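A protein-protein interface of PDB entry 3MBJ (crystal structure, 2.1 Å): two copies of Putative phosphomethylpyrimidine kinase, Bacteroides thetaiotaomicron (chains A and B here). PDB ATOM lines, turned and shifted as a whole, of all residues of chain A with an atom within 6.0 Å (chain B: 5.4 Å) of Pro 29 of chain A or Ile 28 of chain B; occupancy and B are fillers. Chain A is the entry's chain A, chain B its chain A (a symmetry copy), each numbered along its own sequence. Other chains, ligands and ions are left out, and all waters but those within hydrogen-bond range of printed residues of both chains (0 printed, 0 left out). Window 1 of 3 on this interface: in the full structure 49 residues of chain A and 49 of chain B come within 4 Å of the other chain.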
ATOM      1  N   LEU A  16     -10.380  30.105 -12.658  1.00  0.00           N
ATOM      2  CA  LEU A  16     -11.820  29.863 -12.767  1.00  0.00           C
ATOM      3  C   LEU A  16     -12.399  30.999 -13.600  1.00  0.00           C
ATOM      4  O   LEU A  16     -12.320  32.173 -13.205  1.00  0.00           O
ATOM      5  CB  LEU A  16     -12.489  29.769 -11.390  1.00  0.00           C
ATOM      6  CG  LEU A  16     -13.975  29.360 -11.370  1.00  0.00           C
ATOM      7  CD1 LEU A  16     -14.218  27.887 -11.702  1.00  0.00           C
ATOM      8  CD2 LEU A  16     -14.629  29.715 -10.051  1.00  0.00           C
ATOM      9  N   LEU A  24     -10.376  25.804 -15.457  1.00  0.00           N
ATOM     10  CA  LEU A  24     -11.022  24.869 -14.536  1.00  0.00           C
ATOM     11  C   LEU A  24     -12.379  24.381 -14.994  1.00  0.00           C
ATOM     12  O   LEU A  24     -12.791  23.277 -14.578  1.00  0.00           O
ATOM     13  CB  LEU A  24     -11.150  25.434 -13.118  1.00  0.00           C
ATOM     14  CG  LEU A  24      -9.875  25.545 -12.253  1.00  0.00           C
ATOM     15  CD1 LEU A  24     -10.143  26.363 -11.009  1.00  0.00           C
ATOM     16  CD2 LEU A  24      -9.224  24.165 -11.895  1.00  0.00           C
ATOM     17  N   THR A  25     -13.093  25.159 -15.815  1.00  0.00           N
ATOM     18  CA  THR A  25     -14.413  24.709 -16.208  1.00  0.00           C
ATOM     19  C   THR A  25     -14.354  23.669 -17.340  1.00  0.00           C
ATOM     20  O   THR A  25     -15.402  23.098 -17.670  1.00  0.00           O
ATOM     21  CB  THR A  25     -15.381  25.875 -16.510  1.00  0.00           C
ATOM     22  OG1 THR A  25     -14.776  26.731 -17.478  1.00  0.00           O
ATOM     23  CG2 THR A  25     -15.648  26.661 -15.210  1.00  0.00           C
ATOM     24  N   VAL A  26     -13.162  23.426 -17.923  1.00  0.00           N
ATOM     25  CA  VAL A  26     -12.931  22.252 -18.768  1.00  0.00           C
ATOM     26  C   VAL A  26     -12.144  21.148 -18.035  1.00  0.00           C
ATOM     27  O   VAL A  26     -12.540  19.998 -18.047  1.00  0.00           O
ATOM     28  CB  VAL A  26     -12.272  22.598 -20.146  1.00  0.00           C
ATOM     29  CG1 VAL A  26     -12.846  23.873 -20.712  1.00  0.00           C
ATOM     30  CG2 VAL A  26     -10.798  22.671 -20.056  1.00  0.00           C
ATOM     31  N   VAL A  27     -11.080  21.503 -17.331  1.00  0.00           N
ATOM     32  CA  VAL A  27     -10.325  20.541 -16.574  1.00  0.00           C
ATOM     33  C   VAL A  27     -11.224  19.755 -15.613  1.00  0.00           C
ATOM     34  O   VAL A  27     -11.096  18.516 -15.480  1.00  0.00           O
ATOM     35  CB  VAL A  27      -9.167  21.247 -15.752  1.00  0.00           C
ATOM     36  CG1 VAL A  27      -8.374  20.216 -14.948  1.00  0.00           C
ATOM     37  CG2 VAL A  27      -8.219  22.046 -16.675  1.00  0.00           C
ATOM     38  N   ILE A  28     -12.113  20.428 -14.890  1.00  0.00           N
ATOM     39  CA  ILE A  28     -12.886  19.698 -13.867  1.00  0.00           C
ATOM     40  C   ILE A  28     -13.825  18.616 -14.486  1.00  0.00           C
ATOM     41  O   ILE A  28     -13.847  17.468 -14.021  1.00  0.00           O
ATOM     42  CB  ILE A  28     -13.708  20.633 -12.935  1.00  0.00           C
ATOM     43  CG1 ILE A  28     -12.776  21.353 -11.972  1.00  0.00           C
ATOM     44  CG2 ILE A  28     -14.746  19.833 -12.136  1.00  0.00           C
ATOM     45  CD1 ILE A  28     -13.421  22.624 -11.380  1.00  0.00           C
ATOM     46  N   PRO A  29     -14.644  18.995 -15.483  1.00  0.00           N
ATOM     47  CA  PRO A  29     -15.609  17.996 -15.993  1.00  0.00           C
ATOM     48  C   PRO A  29     -14.939  16.894 -16.807  1.00  0.00           C
ATOM     49  O   PRO A  29     -15.306  15.750 -16.680  1.00  0.00           O
ATOM     50  CB  PRO A  29     -16.578  18.824 -16.868  1.00  0.00           C
ATOM     51  CG  PRO A  29     -15.827  20.084 -17.184  1.00  0.00           C
ATOM     52  CD  PRO A  29     -15.017  20.352 -15.915  1.00  0.00           C
ATOM     53  N   ILE A  30     -13.918  17.235 -17.594  1.00  0.00           N
ATOM     54  CA  ILE A  30     -13.179  16.204 -18.276  1.00  0.00           C
ATOM     55  C   ILE A  30     -12.535  15.144 -17.349  1.00  0.00           C
ATOM     56  O   ILE A  30     -12.739  13.932 -17.532  1.00  0.00           O
ATOM     57  CB  ILE A  30     -12.137  16.794 -19.199  1.00  0.00           C
ATOM     58  CG1 ILE A  30     -12.856  17.533 -20.336  1.00  0.00           C
ATOM     59  CG2 ILE A  30     -11.246  15.677 -19.754  1.00  0.00           C
ATOM     60  CD1 ILE A  30     -11.926  18.310 -21.227  1.00  0.00           C
ATOM     61  N   LEU A  31     -11.722  15.574 -16.401  1.00  0.00           N
ATOM     62  CA  LEU A  31     -10.971  14.602 -15.608  1.00  0.00           C
ATOM     63  C   LEU A  31     -11.903  13.879 -14.638  1.00  0.00           C
ATOM     64  O   LEU A  31     -11.736  12.685 -14.392  1.00  0.00           O
ATOM     65  CB  LEU A  31      -9.777  15.234 -14.898  1.00  0.00           C
ATOM     66  CG  LEU A  31      -8.575  15.692 -15.753  1.00  0.00           C
ATOM     67  CD1 LEU A  31      -7.622  16.506 -14.886  1.00  0.00           C
ATOM     68  CD2 LEU A  31      -7.802  14.484 -16.403  1.00  0.00           C
ATOM     69  N   SER A  32     -12.937  14.564 -14.171  1.00  0.00           N
ATOM     70  CA  SER A  32     -13.937  13.890 -13.361  1.00  0.00           C
ATOM     71  C   SER A  32     -14.675  12.804 -14.182  1.00  0.00           C
ATOM     72  O   SER A  32     -14.976  11.698 -13.649  1.00  0.00           O
ATOM     73  CB  SER A  32     -14.902  14.905 -12.797  1.00  0.00           C
ATOM     74  OG  SER A  32     -15.860  14.198 -12.062  1.00  0.00           O
ATOM     75  N   SER A  33     -14.891  13.068 -15.491  1.00  0.00           N
ATOM     76  CA  SER A  33     -15.650  12.113 -16.328  1.00  0.00           C
ATOM     77  C   SER A  33     -14.761  10.914 -16.695  1.00  0.00           C
ATOM     78  O   SER A  33     -15.273   9.841 -17.024  1.00  0.00           O
ATOM     79  CB  SER A  33     -16.260  12.759 -17.588  1.00  0.00           C
ATOM     80  OG  SER A  33     -15.286  13.051 -18.605  1.00  0.00           O
ATOM     81  N   MET A  34     -13.434  11.128 -16.646  1.00  0.00           N
ATOM     82  CA  MET A  34     -12.422  10.094 -16.808  1.00  0.00           C
ATOM     83  C   MET A  34     -12.072   9.316 -15.562  1.00  0.00           C
ATOM     84  O   MET A  34     -11.216   8.457 -15.626  1.00  0.00           O
ATOM     85  CB  MET A  34     -11.151  10.707 -17.477  1.00  0.00           C
ATOM     86  CG  MET A  34     -11.457  11.272 -18.817  1.00  0.00           C
ATOM     87  SD  MET A  34      -9.922  11.922 -19.871  1.00  0.00           S
ATOM     88  CE  MET A  34      -9.396  10.177 -20.378  1.00  0.00           C
ATOM     89  N   VAL A  38     -10.754  16.169  -9.255  1.00  0.00           N
ATOM     90  CA  VAL A  38      -9.991  17.388  -9.533  1.00  0.00           C
ATOM     91  C   VAL A  38     -10.104  18.305  -8.307  1.00  0.00           C
ATOM     92  O   VAL A  38     -11.186  18.617  -7.851  1.00  0.00           O
ATOM     93  CB  VAL A  38     -10.457  18.116 -10.820  1.00  0.00           C
ATOM     94  CG1 VAL A  38      -9.705  19.463 -11.018  1.00  0.00           C
ATOM     95  CG2 VAL A  38     -10.310  17.234 -12.068  1.00  0.00           C
ATOM     96  N   LEU A 272     -18.261  21.115 -25.623  1.00  0.00           N
ATOM     97  CA  LEU A 272     -17.745  20.014 -24.878  1.00  0.00           C
ATOM     98  C   LEU A 272     -18.800  19.034 -24.383  1.00  0.00           C
ATOM     99  O   LEU A 272     -18.582  17.814 -24.398  1.00  0.00           O
ATOM    100  CB  LEU A 272     -17.049  20.585 -23.648  1.00  0.00           C
ATOM    101  CG  LEU A 272     -16.318  19.653 -22.699  1.00  0.00           C
ATOM    102  CD1 LEU A 272     -15.347  18.747 -23.489  1.00  0.00           C
ATOM    103  CD2 LEU A 272     -15.554  20.501 -21.652  1.00  0.00           C
ATOM    104  N   LEU A 276     -18.515  14.982 -24.378  1.00  0.00           N
ATOM    105  CA  LEU A 276     -17.865  14.425 -23.192  1.00  0.00           C
ATOM    106  C   LEU A 276     -17.925  12.890 -23.127  1.00  0.00           C
ATOM    107  O   LEU A 276     -16.925  12.225 -22.757  1.00  0.00           O
ATOM    108  CB  LEU A 276     -18.529  14.949 -21.939  1.00  0.00           C
ATOM    109  CG  LEU A 276     -17.734  14.947 -20.657  1.00  0.00           C
ATOM    110  CD1 LEU A 276     -16.340  15.632 -20.830  1.00  0.00           C
ATOM    111  CD2 LEU A 276     -18.565  15.722 -19.606  1.00  0.00           C
ATOM    112  N   LEU B  16     -16.327  27.744  -4.507  1.00  0.00           N
ATOM    113  CA  LEU B  16     -15.302  26.840  -5.034  1.00  0.00           C
ATOM    114  C   LEU B  16     -14.489  26.350  -3.843  1.00  0.00           C
ATOM    115  O   LEU B  16     -13.851  27.152  -3.142  1.00  0.00           O
ATOM    116  CB  LEU B  16     -14.418  27.527  -6.082  1.00  0.00           C
ATOM    117  CG  LEU B  16     -13.404  26.632  -6.824  1.00  0.00           C
ATOM    118  CD1 LEU B  16     -14.041  25.681  -7.836  1.00  0.00           C
ATOM    119  CD2 LEU B  16     -12.323  27.459  -7.489  1.00  0.00           C
ATOM    120  N   SER B  23     -20.558  21.914  -3.552  1.00  0.00           N
ATOM    121  CA  SER B  23     -20.636  23.171  -4.276  1.00  0.00           C
ATOM    122  C   SER B  23     -20.136  23.017  -5.724  1.00  0.00           C
ATOM    123  O   SER B  23     -20.539  22.076  -6.403  1.00  0.00           O
ATOM    124  CB  SER B  23     -19.933  24.332  -3.502  1.00  0.00           C
ATOM    125  OG  SER B  23     -18.520  24.108  -3.346  1.00  0.00           O
ATOM    126  N   LEU B  24     -19.280  23.911  -6.216  1.00  0.00           N
ATOM    127  CA  LEU B  24     -18.967  23.931  -7.645  1.00  0.00           C
ATOM    128  C   LEU B  24     -18.231  22.703  -8.138  1.00  0.00           C
ATOM    129  O   LEU B  24     -18.335  22.385  -9.343  1.00  0.00           O
ATOM    130  CB  LEU B  24     -18.181  25.179  -8.058  1.00  0.00           C
ATOM    131  CG  LEU B  24     -18.925  26.532  -8.112  1.00  0.00           C
ATOM    132  CD1 LEU B  24     -17.946  27.674  -8.269  1.00  0.00           C
ATOM    133  CD2 LEU B  24     -20.052  26.597  -9.198  1.00  0.00           C
ATOM    134  N   THR B  25     -17.485  22.014  -7.267  1.00  0.00           N
ATOM    135  CA  THR B  25     -16.742  20.870  -7.757  1.00  0.00           C
ATOM    136  C   THR B  25     -17.632  19.622  -7.895  1.00  0.00           C
ATOM    137  O   THR B  25     -17.155  18.617  -8.438  1.00  0.00           O
ATOM    138  CB  THR B  25     -15.448  20.605  -6.957  1.00  0.00           C
ATOM    139  OG1 THR B  25     -15.782  20.497  -5.574  1.00  0.00           O
ATOM    140  CG2 THR B  25     -14.471  21.778  -7.171  1.00  0.00           C
ATOM    141  N   VAL B  26     -18.891  19.679  -7.415  1.00  0.00           N
ATOM    142  CA  VAL B  26     -19.908  18.686  -7.770  1.00  0.00           C
ATOM    143  C   VAL B  26     -20.902  19.216  -8.821  1.00  0.00           C
ATOM    144  O   VAL B  26     -21.162  18.560  -9.811  1.00  0.00           O
ATOM    145  CB  VAL B  26     -20.658  18.092  -6.531  1.00  0.00           C
ATOM    146  CG1 VAL B  26     -19.703  17.864  -5.383  1.00  0.00           C
ATOM    147  CG2 VAL B  26     -21.800  18.932  -6.114  1.00  0.00           C
ATOM    148  N   VAL B  27     -21.396  20.435  -8.654  1.00  0.00           N
ATOM    149  CA  VAL B  27     -22.287  21.023  -9.618  1.00  0.00           C
ATOM    150  C   VAL B  27     -21.680  21.003 -11.026  1.00  0.00           C
ATOM    151  O   VAL B  27     -22.372  20.686 -12.020  1.00  0.00           O
ATOM    152  CB  VAL B  27     -22.647  22.516  -9.221  1.00  0.00           C
ATOM    153  CG1 VAL B  27     -23.591  23.133 -10.254  1.00  0.00           C
ATOM    154  CG2 VAL B  27     -23.278  22.594  -7.812  1.00  0.00           C
ATOM    155  N   ILE B  28     -20.412  21.375 -11.169  1.00  0.00           N
ATOM    156  CA  ILE B  28     -19.863  21.489 -12.534  1.00  0.00           C
ATOM    157  C   ILE B  28     -19.813  20.116 -13.274  1.00  0.00           C
ATOM    158  O   ILE B  28     -20.246  20.016 -14.432  1.00  0.00           O
ATOM    159  CB  ILE B  28     -18.459  22.157 -12.577  1.00  0.00           C
ATOM    160  CG1 ILE B  28     -18.589  23.650 -12.313  1.00  0.00           C
ATOM    161  CG2 ILE B  28     -17.792  21.938 -13.941  1.00  0.00           C
ATOM    162  CD1 ILE B  28     -17.255  24.277 -11.853  1.00  0.00           C
ATOM    163  N   PRO B  29     -19.233  19.084 -12.641  1.00  0.00           N
ATOM    164  CA  PRO B  29     -19.089  17.814 -13.387  1.00  0.00           C
ATOM    165  C   PRO B  29     -20.420  17.095 -13.584  1.00  0.00           C
ATOM    166  O   PRO B  29     -20.662  16.561 -14.640  1.00  0.00           O
ATOM    167  CB  PRO B  29     -18.125  16.975 -12.519  1.00  0.00           C
ATOM    168  CG  PRO B  29     -18.191  17.601 -11.157  1.00  0.00           C
ATOM    169  CD  PRO B  29     -18.364  19.091 -11.452  1.00  0.00           C
ATOM    170  N   ILE B  30     -21.303  17.136 -12.584  1.00  0.00           N
ATOM    171  CA  ILE B  30     -22.616  16.581 -12.781  1.00  0.00           C
ATOM    172  C   ILE B  30     -23.418  17.206 -13.949  1.00  0.00           C
ATOM    173  O   ILE B  30     -23.914  16.490 -14.835  1.00  0.00           O
ATOM    174  CB  ILE B  30     -23.429  16.625 -11.507  1.00  0.00           C
ATOM    175  CG1 ILE B  30     -22.786  15.675 -10.487  1.00  0.00           C
ATOM    176  CG2 ILE B  30     -24.875  16.211 -11.801  1.00  0.00           C
ATOM    177  CD1 ILE B  30     -23.404  15.760  -9.118  1.00  0.00           C
ATOM    178  N   LEU B  31     -23.601  18.514 -13.934  1.00  0.00           N
ATOM    179  CA  LEU B  31     -24.484  19.125 -14.928  1.00  0.00           C
ATOM    180  C   LEU B  31     -23.815  19.121 -16.300  1.00  0.00           C
ATOM    181  O   LEU B  31     -24.484  18.928 -17.315  1.00  0.00           O
ATOM    182  CB  LEU B  31     -24.942  20.520 -14.514  1.00  0.00           C
ATOM    183  CG  LEU B  31     -25.933  20.646 -13.335  1.00  0.00           C
ATOM    184  CD1 LEU B  31     -26.059  22.111 -12.939  1.00  0.00           C
ATOM    185  CD2 LEU B  31     -27.354  20.063 -13.677  1.00  0.00           C
ATOM    186  N   SER B  32     -22.494  19.226 -16.329  1.00  0.00           N
ATOM    187  CA  SER B  32     -21.790  19.082 -17.593  1.00  0.00           C
ATOM    188  C   SER B  32     -21.964  17.655 -18.165  1.00  0.00           C
ATOM    189  O   SER B  32     -22.127  17.482 -19.407  1.00  0.00           O
ATOM    190  CB  SER B  32     -20.333  19.427 -17.403  1.00  0.00           C
ATOM    191  OG  SER B  32     -19.701  19.234 -18.636  1.00  0.00           O
ATOM    192  N   SER B  33     -22.020  16.640 -17.271  1.00  0.00           N
ATOM    193  CA  SER B  33     -22.115  15.240 -17.740  1.00  0.00           C
ATOM    194  C   SER B  33     -23.549  14.938 -18.206  1.00  0.00           C
ATOM    195  O   SER B  33     -23.763  14.007 -18.987  1.00  0.00           O
ATOM    196  CB  SER B  33     -21.644  14.214 -16.691  1.00  0.00           C
ATOM    197  OG  SER B  33     -22.576  14.034 -15.611  1.00  0.00           O
ATOM    198  N   VAL B  38     -22.096  24.741 -17.299  1.00  0.00           N
ATOM    199  CA  VAL B  38     -22.182  25.387 -15.987  1.00  0.00           C
ATOM    200  C   VAL B  38     -21.285  26.632 -16.015  1.00  0.00           C
ATOM    201  O   VAL B  38     -20.116  26.559 -16.339  1.00  0.00           O
ATOM    202  CB  VAL B  38     -21.794  24.443 -14.820  1.00  0.00           C
ATOM    203  CG1 VAL B  38     -21.785  25.196 -13.458  1.00  0.00           C
ATOM    204  CG2 VAL B  38     -22.707  23.212 -14.743  1.00  0.00           C
ATOM    205  N   PRO B  40     -19.933  29.320 -13.681  1.00  0.00           N
ATOM    206  CA  PRO B  40     -19.833  29.649 -12.253  1.00  0.00           C
ATOM    207  C   PRO B  40     -19.810  31.154 -11.962  1.00  0.00           C
ATOM    208  O   PRO B  40     -19.111  31.929 -12.639  1.00  0.00           O
ATOM    209  CB  PRO B  40     -18.479  29.046 -11.859  1.00  0.00           C
ATOM    210  CG  PRO B  40     -17.695  29.155 -13.091  1.00  0.00           C
ATOM    211  CD  PRO B  40     -18.630  28.910 -14.230  1.00  0.00           C
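O of Pro 29 of chain B lies close to OG of Ser 33 of chain B (3.3 Å).
The side-chain hydroxyl of Ser 33 of chain A lies close to the backbone carbonyl oxygen of Pro 29 of chain A (3.3 Å).
CD1 of Leu 16 of chain A touches CG of Pro 40 of chain B, at 3.95 Å.
Thr 25 of chain A touches Pro 40 of chain B.
Pro 29 of chain B touches Ile 28 of chain A (CD to CG2, 3.8 Å).
Ile 28 of chain B touches Pro 29 of chain A.
Pro 29 of chain A touches Ser 32 of chain B.
Pro 29 of chain B touches Ser 32 of chain A (CB to OG, 3.6 Å).
Leu 276 of chain A touches Ser 32 of chain B (CD2 to OG, 3.8 Å).
Of the printed residues of chain A, Ile 28 of chain B touches Pro 29.
Of the printed residues of chain B, Thr 25 of chain A touches Pro 40 (3.9 Å).
Of the printed residues of chain A, Ser 32 of chain B touches Pro 29 and Leu 276.
Of the printed residues of chain B, Leu 276 of chain A touches Ser 32.
Of the printed residues of chain B, Ile 28 of chain A touches Pro 29 (3.8 Å).
Of the printed residues of chain B, Leu 16 of chain A touches Pro 40.
Val 26 of chain B touches none of the printed residues of chain A.
The nearest residue of chain A that does not touch Ile 28 of chain B is Ile 28 of chain A (4.1 Å).
The nearest printed residue of chain A that does not touch Pro 40 of chain B is Leu 24 of chain A (7.4 Å).
Of the 15 printed residues of chain A, 6 touch a printed residue of chain B.
Of the 14 printed residues of chain B, 4 touch a printed residue of chain A.
Among the printed residues, 7 pairs touch across the chains.
Among the printed residues, no Asp or Glu carboxylate lies within 4 Å of a Lys or Arg side-chain nitrogen of the other chain.
Ile 28 of chain A touches Pro 29 of chain B, and with the chains exchanged Pro 29 of chain A touches Ile 28 of chain B.
Pro 29 of chain A touches Ser 32 of chain B, and with the chains exchanged Ser 32 of chain A touches Pro 29 of chain B.
Positions printed for both chains: 16, 24, 25, 26, 27, 28, 29, 30, 31, 32, 33 and 38.
Of the 7 pairs that touch across the chains among the printed residues, 4 have their exchanged pair printed and touching as well.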
